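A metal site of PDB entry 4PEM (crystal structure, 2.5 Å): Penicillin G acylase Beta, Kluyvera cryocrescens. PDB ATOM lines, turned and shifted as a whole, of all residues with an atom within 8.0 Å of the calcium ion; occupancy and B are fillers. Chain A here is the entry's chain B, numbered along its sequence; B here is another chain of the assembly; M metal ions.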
ATOM      1  N   GLY A  75      -5.386 -16.728  18.934  1.00  0.00           N
ATOM      2  CA  GLY A  75      -5.209 -16.149  17.608  1.00  0.00           C
ATOM      3  C   GLY A  75      -3.766 -16.310  17.159  1.00  0.00           C
ATOM      4  O   GLY A  75      -2.861 -16.496  17.990  1.00  0.00           O
ATOM      5  N   ASP A  76      -3.528 -16.267  15.853  1.00  0.00           N
ATOM      6  CA  ASP A  76      -2.172 -16.330  15.364  1.00  0.00           C
ATOM      7  C   ASP A  76      -1.517 -14.942  15.537  1.00  0.00           C
ATOM      8  O   ASP A  76      -1.685 -14.052  14.690  1.00  0.00           O
ATOM      9  CB  ASP A  76      -2.112 -16.822  13.906  1.00  0.00           C
ATOM     10  CG  ASP A  76      -0.724 -17.315  13.507  1.00  0.00           C
ATOM     11  OD1 ASP A  76       0.290 -16.841  14.098  1.00  0.00           O
ATOM     12  OD2 ASP A  76      -0.610 -18.196  12.615  1.00  0.00           O
ATOM     13  N   ASP A  77      -0.780 -14.779  16.636  1.00  0.00           N
ATOM     14  CA  ASP A  77      -0.027 -13.552  16.935  1.00  0.00           C
ATOM     15  C   ASP A  77       1.450 -13.836  16.974  1.00  0.00           C
ATOM     16  O   ASP A  77       2.251 -13.019  17.467  1.00  0.00           O
ATOM     17  CB  ASP A  77      -0.492 -12.916  18.264  1.00  0.00           C
ATOM     18  CG  ASP A  77      -0.377 -13.875  19.472  1.00  0.00           C
ATOM     19  OD1 ASP A  77       0.058 -15.019  19.295  1.00  0.00           O
ATOM     20  OD2 ASP A  77      -0.756 -13.478  20.598  1.00  0.00           O
ATOM     21  N   VAL A  78       1.811 -14.999  16.448  1.00  0.00           N
ATOM     22  CA  VAL A  78       3.197 -15.470  16.475  1.00  0.00           C
ATOM     23  C   VAL A  78       3.503 -16.211  15.182  1.00  0.00           C
ATOM     24  O   VAL A  78       2.798 -17.136  14.789  1.00  0.00           O
ATOM     25  CB  VAL A  78       3.476 -16.437  17.641  1.00  0.00           C
ATOM     26  CG1 VAL A  78       4.915 -16.919  17.614  1.00  0.00           C
ATOM     27  CG2 VAL A  78       3.208 -15.752  18.967  1.00  0.00           C
ATOM     28  N   ASP A  79       4.586 -15.799  14.542  1.00  0.00           N
ATOM     29  CA  ASP A  79       5.050 -16.402  13.310  1.00  0.00           C
ATOM     30  C   ASP A  79       6.552 -16.642  13.415  1.00  0.00           C
ATOM     31  O   ASP A  79       7.238 -16.006  14.181  1.00  0.00           O
ATOM     32  CB  ASP A  79       4.739 -15.477  12.130  1.00  0.00           C
ATOM     33  CG  ASP A  79       3.254 -15.449  11.780  1.00  0.00           C
ATOM     34  OD1 ASP A  79       2.523 -16.407  12.157  1.00  0.00           O
ATOM     35  OD2 ASP A  79       2.834 -14.481  11.112  1.00  0.00           O
ATOM     36  N   ILE A  80       7.025 -17.581  12.620  1.00  0.00           N
ATOM     37  CA  ILE A  80       8.391 -18.010  12.701  1.00  0.00           C
ATOM     38  C   ILE A  80       9.156 -17.656  11.439  1.00  0.00           C
ATOM     39  O   ILE A  80       8.800 -18.070  10.335  1.00  0.00           O
ATOM     40  CB  ILE A  80       8.430 -19.519  13.020  1.00  0.00           C
ATOM     41  CG1 ILE A  80       8.074 -19.685  14.506  1.00  0.00           C
ATOM     42  CG2 ILE A  80       9.790 -20.118  12.726  1.00  0.00           C
ATOM     43  CD1 ILE A  80       7.863 -21.107  14.971  1.00  0.00           C
ATOM     44  N   ALA A 143       8.795 -14.670  16.222  1.00  0.00           N
ATOM     45  CA  ALA A 143       8.215 -13.341  16.092  1.00  0.00           C
ATOM     46  C   ALA A 143       6.814 -13.278  16.694  1.00  0.00           C
ATOM     47  O   ALA A 143       5.894 -13.982  16.261  1.00  0.00           O
ATOM     48  CB  ALA A 143       8.155 -12.937  14.657  1.00  0.00           C
ATOM     49  N   PRO A 200      -0.214  -9.132  13.596  1.00  0.00           N
ATOM     50  CA  PRO A 200       0.690  -8.629  12.581  1.00  0.00           C
ATOM     51  C   PRO A 200      -0.048  -8.347  11.284  1.00  0.00           C
ATOM     52  O   PRO A 200      -0.962  -9.096  10.926  1.00  0.00           O
ATOM     53  CB  PRO A 200       1.657  -9.796  12.382  1.00  0.00           C
ATOM     54  CG  PRO A 200       0.793 -11.003  12.599  1.00  0.00           C
ATOM     55  CD  PRO A 200      -0.193 -10.609  13.659  1.00  0.00           C
ATOM     56  N   ARG A 202       0.381  -8.812   7.716  1.00  0.00           N
ATOM     57  CA  ARG A 202       1.222  -9.699   6.940  1.00  0.00           C
ATOM     58  C   ARG A 202       1.238  -9.302   5.476  1.00  0.00           C
ATOM     59  O   ARG A 202       0.294  -8.666   4.989  1.00  0.00           O
ATOM     60  CB  ARG A 202       0.756 -11.156   7.083  1.00  0.00           C
ATOM     61  CG  ARG A 202       1.014 -11.805   8.441  1.00  0.00           C
ATOM     62  CD  ARG A 202       0.400 -13.212   8.516  1.00  0.00           C
ATOM     63  NE  ARG A 202       0.660 -13.879   9.803  1.00  0.00           N
ATOM     64  CZ  ARG A 202      -0.184 -13.903  10.830  1.00  0.00           C
ATOM     65  NH1 ARG A 202      -1.385 -13.327  10.747  1.00  0.00           N
ATOM     66  NH2 ARG A 202       0.148 -14.525  11.959  1.00  0.00           N
ATOM     67  N   HIS A 206       1.452 -14.566   2.515  1.00  0.00           N
ATOM     68  CA  HIS A 206       1.953 -15.105   3.781  1.00  0.00           C
ATOM     69  C   HIS A 206       0.970 -16.145   4.342  1.00  0.00           C
ATOM     70  O   HIS A 206      -0.080 -15.795   4.892  1.00  0.00           O
ATOM     71  CB  HIS A 206       2.135 -13.971   4.804  1.00  0.00           C
ATOM     72  CG  HIS A 206       2.868 -14.364   6.045  1.00  0.00           C
ATOM     73  ND1 HIS A 206       2.632 -15.548   6.720  1.00  0.00           N
ATOM     74  CD2 HIS A 206       3.815 -13.708   6.757  1.00  0.00           C
ATOM     75  CE1 HIS A 206       3.454 -15.631   7.753  1.00  0.00           C
ATOM     76  NE2 HIS A 206       4.180 -14.515   7.802  1.00  0.00           N
ATOM     77  N   ASP A 207       1.357 -17.405   4.268  1.00  0.00           N
ATOM     78  CA  ASP A 207       0.682 -18.479   4.985  1.00  0.00           C
ATOM     79  C   ASP A 207       1.112 -18.553   6.465  1.00  0.00           C
ATOM     80  O   ASP A 207       2.203 -19.006   6.752  1.00  0.00           O
ATOM     81  CB  ASP A 207       0.986 -19.816   4.295  1.00  0.00           C
ATOM     82  CG  ASP A 207       0.258 -20.974   4.924  1.00  0.00           C
ATOM     83  OD1 ASP A 207      -0.331 -20.807   6.015  1.00  0.00           O
ATOM     84  OD2 ASP A 207       0.298 -22.067   4.332  1.00  0.00           O
ATOM     85  N   PRO A 208       0.211 -18.195   7.403  1.00  0.00           N
ATOM     86  CA  PRO A 208       0.525 -18.120   8.837  1.00  0.00           C
ATOM     87  C   PRO A 208       0.703 -19.452   9.567  1.00  0.00           C
ATOM     88  O   PRO A 208       1.192 -19.464  10.700  1.00  0.00           O
ATOM     89  CB  PRO A 208      -0.670 -17.346   9.396  1.00  0.00           C
ATOM     90  CG  PRO A 208      -1.798 -17.675   8.508  1.00  0.00           C
ATOM     91  CD  PRO A 208      -1.197 -17.864   7.145  1.00  0.00           C
ATOM     92  N   ARG A 209       0.336 -20.552   8.932  1.00  0.00           N
ATOM     93  CA  ARG A 209       0.528 -21.881   9.510  1.00  0.00           C
ATOM     94  C   ARG A 209       1.969 -22.371   9.403  1.00  0.00           C
ATOM     95  O   ARG A 209       2.323 -23.339  10.072  1.00  0.00           O
ATOM     96  CB  ARG A 209      -0.334 -22.911   8.834  1.00  0.00           C
ATOM     97  CG  ARG A 209      -1.719 -22.471   8.414  1.00  0.00           C
ATOM     98  CD  ARG A 209      -2.615 -23.709   8.289  1.00  0.00           C
ATOM     99  NE  ARG A 209      -3.241 -24.074   6.996  1.00  0.00           N
ATOM    100  CZ  ARG A 209      -2.695 -24.003   5.786  1.00  0.00           C
ATOM    101  NH1 ARG A 209      -1.471 -23.560   5.568  1.00  0.00           N
ATOM    102  NH2 ARG A 209      -3.407 -24.385   4.753  1.00  0.00           N
ATOM    103  N   LEU A 210       2.807 -21.758   8.578  1.00  0.00           N
ATOM    104  CA  LEU A 210       4.183 -22.271   8.365  1.00  0.00           C
ATOM    105  C   LEU A 210       5.215 -21.138   8.417  1.00  0.00           C
ATOM    106  O   LEU A 210       4.871 -19.975   8.221  1.00  0.00           O
ATOM    107  CB  LEU A 210       4.284 -23.014   7.021  1.00  0.00           C
ATOM    108  CG  LEU A 210       3.522 -24.359   7.040  1.00  0.00           C
ATOM    109  CD1 LEU A 210       3.024 -24.765   5.669  1.00  0.00           C
ATOM    110  CD2 LEU A 210       4.389 -25.448   7.624  1.00  0.00           C
ATOM    111  N   PRO A 211       6.479 -21.486   8.709  1.00  0.00           N
ATOM    112  CA  PRO A 211       7.492 -20.405   8.800  1.00  0.00           C
ATOM    113  C   PRO A 211       7.543 -19.605   7.503  1.00  0.00           C
ATOM    114  O   PRO A 211       6.938 -20.028   6.508  1.00  0.00           O
ATOM    115  CB  PRO A 211       8.808 -21.155   9.016  1.00  0.00           C
ATOM    116  CG  PRO A 211       8.421 -22.482   9.542  1.00  0.00           C
ATOM    117  CD  PRO A 211       7.074 -22.815   8.962  1.00  0.00           C
ATOM    118  N   TRP A 220       6.779  -8.505   8.402  1.00  0.00           N
ATOM    119  CA  TRP A 220       5.504  -7.894   8.697  1.00  0.00           C
ATOM    120  C   TRP A 220       5.542  -6.403   8.358  1.00  0.00           C
ATOM    121  O   TRP A 220       6.572  -5.715   8.526  1.00  0.00           O
ATOM    122  CB  TRP A 220       5.192  -8.048  10.185  1.00  0.00           C
ATOM    123  CG  TRP A 220       4.920  -9.434  10.648  1.00  0.00           C
ATOM    124  CD1 TRP A 220       4.511 -10.513   9.892  1.00  0.00           C
ATOM    125  CD2 TRP A 220       4.958  -9.884  11.994  1.00  0.00           C
ATOM    126  NE1 TRP A 220       4.332 -11.606  10.705  1.00  0.00           N
ATOM    127  CE2 TRP A 220       4.593 -11.255  11.999  1.00  0.00           C
ATOM    128  CE3 TRP A 220       5.259  -9.245  13.222  1.00  0.00           C
ATOM    129  CZ2 TRP A 220       4.528 -12.010  13.147  1.00  0.00           C
ATOM    130  CZ3 TRP A 220       5.194 -10.010  14.380  1.00  0.00           C
ATOM    131  CH2 TRP A 220       4.830 -11.388  14.327  1.00  0.00           C
ATOM    132  N   ALA A 253      -7.532 -19.218  13.198  1.00  0.00           N
ATOM    133  CA  ALA A 253      -7.001 -19.671  14.482  1.00  0.00           C
ATOM    134  C   ALA A 253      -5.481 -19.590  14.607  1.00  0.00           C
ATOM    135  O   ALA A 253      -4.763 -19.236  13.674  1.00  0.00           O
ATOM    136  CB  ALA A 253      -7.453 -21.096  14.741  1.00  0.00           C
ATOM    137  N   SER A 254      -4.988 -19.903  15.793  1.00  0.00           N
ATOM    138  CA  SER A 254      -3.563 -20.036  16.002  1.00  0.00           C
ATOM    139  C   SER A 254      -3.059 -21.190  15.175  1.00  0.00           C
ATOM    140  O   SER A 254      -3.819 -22.123  14.878  1.00  0.00           O
ATOM    141  CB  SER A 254      -3.252 -20.314  17.465  1.00  0.00           C
ATOM    142  OG  SER A 254      -3.193 -21.693  17.713  1.00  0.00           O
ATOM    143  N   ASP A 255      -1.786 -21.147  14.822  1.00  0.00           N
ATOM    144  CA  ASP A 255      -1.182 -22.131  13.905  1.00  0.00           C
ATOM    145  C   ASP A 255      -0.910 -23.515  14.515  1.00  0.00           C
ATOM    146  O   ASP A 255      -0.410 -24.401  13.858  1.00  0.00           O
ATOM    147  CB  ASP A 255       0.091 -21.546  13.280  1.00  0.00           C
ATOM    148  CG  ASP A 255       1.104 -21.127  14.306  1.00  0.00           C
ATOM    149  OD1 ASP A 255       1.416 -21.984  15.166  1.00  0.00           O
ATOM    150  OD2 ASP A 255       1.587 -19.939  14.228  1.00  0.00           O
ATOM    151  N   LEU A 256      -1.274 -23.700  15.778  1.00  0.00           N
ATOM    152  CA  LEU A 256      -1.026 -24.935  16.515  1.00  0.00           C
ATOM    153  C   LEU A 256      -1.680 -26.125  15.852  1.00  0.00           C
ATOM    154  O   LEU A 256      -2.894 -26.178  15.721  1.00  0.00           O
ATOM    155  CB  LEU A 256      -1.550 -24.799  17.955  1.00  0.00           C
ATOM    156  CG  LEU A 256      -0.682 -25.302  19.088  1.00  0.00           C
ATOM    157  CD1 LEU A 256      -1.437 -25.087  20.397  1.00  0.00           C
ATOM    158  CD2 LEU A 256      -0.299 -26.771  18.907  1.00  0.00           C
ATOM    159  N   SER B 175       1.557 -19.466  21.547  1.00  0.00           N
ATOM    160  CA  SER B 175       1.260 -20.808  21.078  1.00  0.00           C
ATOM    161  C   SER B 175       1.562 -20.909  19.597  1.00  0.00           C
ATOM    162  O   SER B 175       0.800 -20.417  18.770  1.00  0.00           O
ATOM    163  CB  SER B 175      -0.215 -21.222  21.330  1.00  0.00           C
ATOM    164  OG  SER B 175      -0.872 -20.357  22.256  1.00  0.00           O
ATOM    165  N   THR B 176       2.642 -21.608  19.253  1.00  0.00           N
ATOM    166  CA  THR B 176       2.941 -21.906  17.862  1.00  0.00           C
ATOM    167  C   THR B 176       3.513 -23.324  17.733  1.00  0.00           C
ATOM    168  O   THR B 176       4.166 -23.819  18.651  1.00  0.00           O
ATOM    169  CB  THR B 176       3.912 -20.842  17.276  1.00  0.00           C
ATOM    170  OG1 THR B 176       3.916 -20.893  15.842  1.00  0.00           O
ATOM    171  CG2 THR B 176       5.330 -20.987  17.823  1.00  0.00           C
ATOM    172  N   SER B 177       3.283 -23.960  16.600  1.00  0.00           N
ATOM    173  CA  SER B 177       3.973 -25.198  16.278  1.00  0.00           C
ATOM    174  C   SER B 177       4.415 -25.174  14.835  1.00  0.00           C
ATOM    175  O   SER B 177       4.490 -26.207  14.193  1.00  0.00           O
ATOM    176  CB  SER B 177       3.037 -26.396  16.516  1.00  0.00           C
ATOM    177  OG  SER B 177       1.894 -26.291  15.696  1.00  0.00           O
ATOM    178  N   GLU B 178       4.734 -23.985  14.318  1.00  0.00           N
ATOM    179  CA  GLU B 178       5.090 -23.842  12.918  1.00  0.00           C
ATOM    180  C   GLU B 178       6.270 -24.762  12.566  1.00  0.00           C
ATOM    181  O   GLU B 178       6.249 -25.382  11.488  1.00  0.00           O
ATOM    182  CB  GLU B 178       5.395 -22.383  12.544  1.00  0.00           C
ATOM    183  CG  GLU B 178       4.175 -21.458  12.407  1.00  0.00           C
ATOM    184  CD  GLU B 178       4.519 -19.992  12.111  1.00  0.00           C
ATOM    185  OE1 GLU B 178       5.687 -19.678  11.726  1.00  0.00           O
ATOM    186  OE2 GLU B 178       3.635 -19.116  12.269  1.00  0.00           O
ATOM    187  N   ASN B 181       4.965 -28.021  12.276  1.00  0.00           N
ATOM    188  CA  ASN B 181       4.110 -28.017  11.098  1.00  0.00           C
ATOM    189  C   ASN B 181       4.882 -28.265   9.815  1.00  0.00           C
ATOM    190  O   ASN B 181       4.404 -28.975   8.916  1.00  0.00           O
ATOM    191  CB  ASN B 181       3.373 -26.691  10.988  1.00  0.00           C
ATOM    192  CG  ASN B 181       2.364 -26.464  12.098  1.00  0.00           C
ATOM    193  OD1 ASN B 181       2.270 -27.235  13.034  1.00  0.00           O
ATOM    194  ND2 ASN B 181       1.565 -25.416  11.953  1.00  0.00           N
HETATM  195 CA    CA M   1       1.747 -18.192  12.708  1.00  0.00          CA
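OD2 of Asp 79 lies within salt-bridge range of NE of Arg 202 (2.6 Å).
OD2 of Asp 79 lies within hydrogen-bond range of NE1 of Trp 220 (3.3 Å).
The backbone NH (N) of Asp 79 is in hydrogen-bond range of the backbone carbonyl oxygen (O) of Ala 143, at 2.8 Å.
OE1 of Glu 178 of chain B is in hydrogen-bond range of N of Ile 80, 2.6 Å away.
OD1 of Asp 255 lies within hydrogen-bond range of OG1 of Thr 176 of chain B (2.8 Å).
The backbone NH (N) of Ser 177 of chain B lies within hydrogen-bond range of the side-chain carboxylate (OD1) of Asp 255.
ND2 of Asn 181 of chain B lies within hydrogen-bond range of O of Asp 255, 2.9 Å away.
O of Asp 76 lies close to NH2 of Arg 202, 3.3 Å away.
Within 4 Å of the calcium ion: Asp 76, Val 78, Asp 79, Pro 208, Asp 255 and Glu 178 of chain B.
The nearest printed residue that does not touch the calcium ion is Arg 202 (4.1 Å).
The calcium ion is bound by the side-chain carboxylate (OD1) of Asp 79 (2.0 Å), the side-chain carboxylate (OE2) of Glu 178 of chain B (2.1 Å), the side-chain carboxylate (OD2) of Asp 255 (2.3 Å), the side-chain carboxylate (OD2) of Asp 76 (2.4 Å), the side-chain carboxylate (OD1) of Asp 76 (2.4 Å), the backbone carbonyl oxygen (O) of Pro 208 (2.4 Å) and the backbone carbonyl oxygen (O) of Val 78 (2.6 Å).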
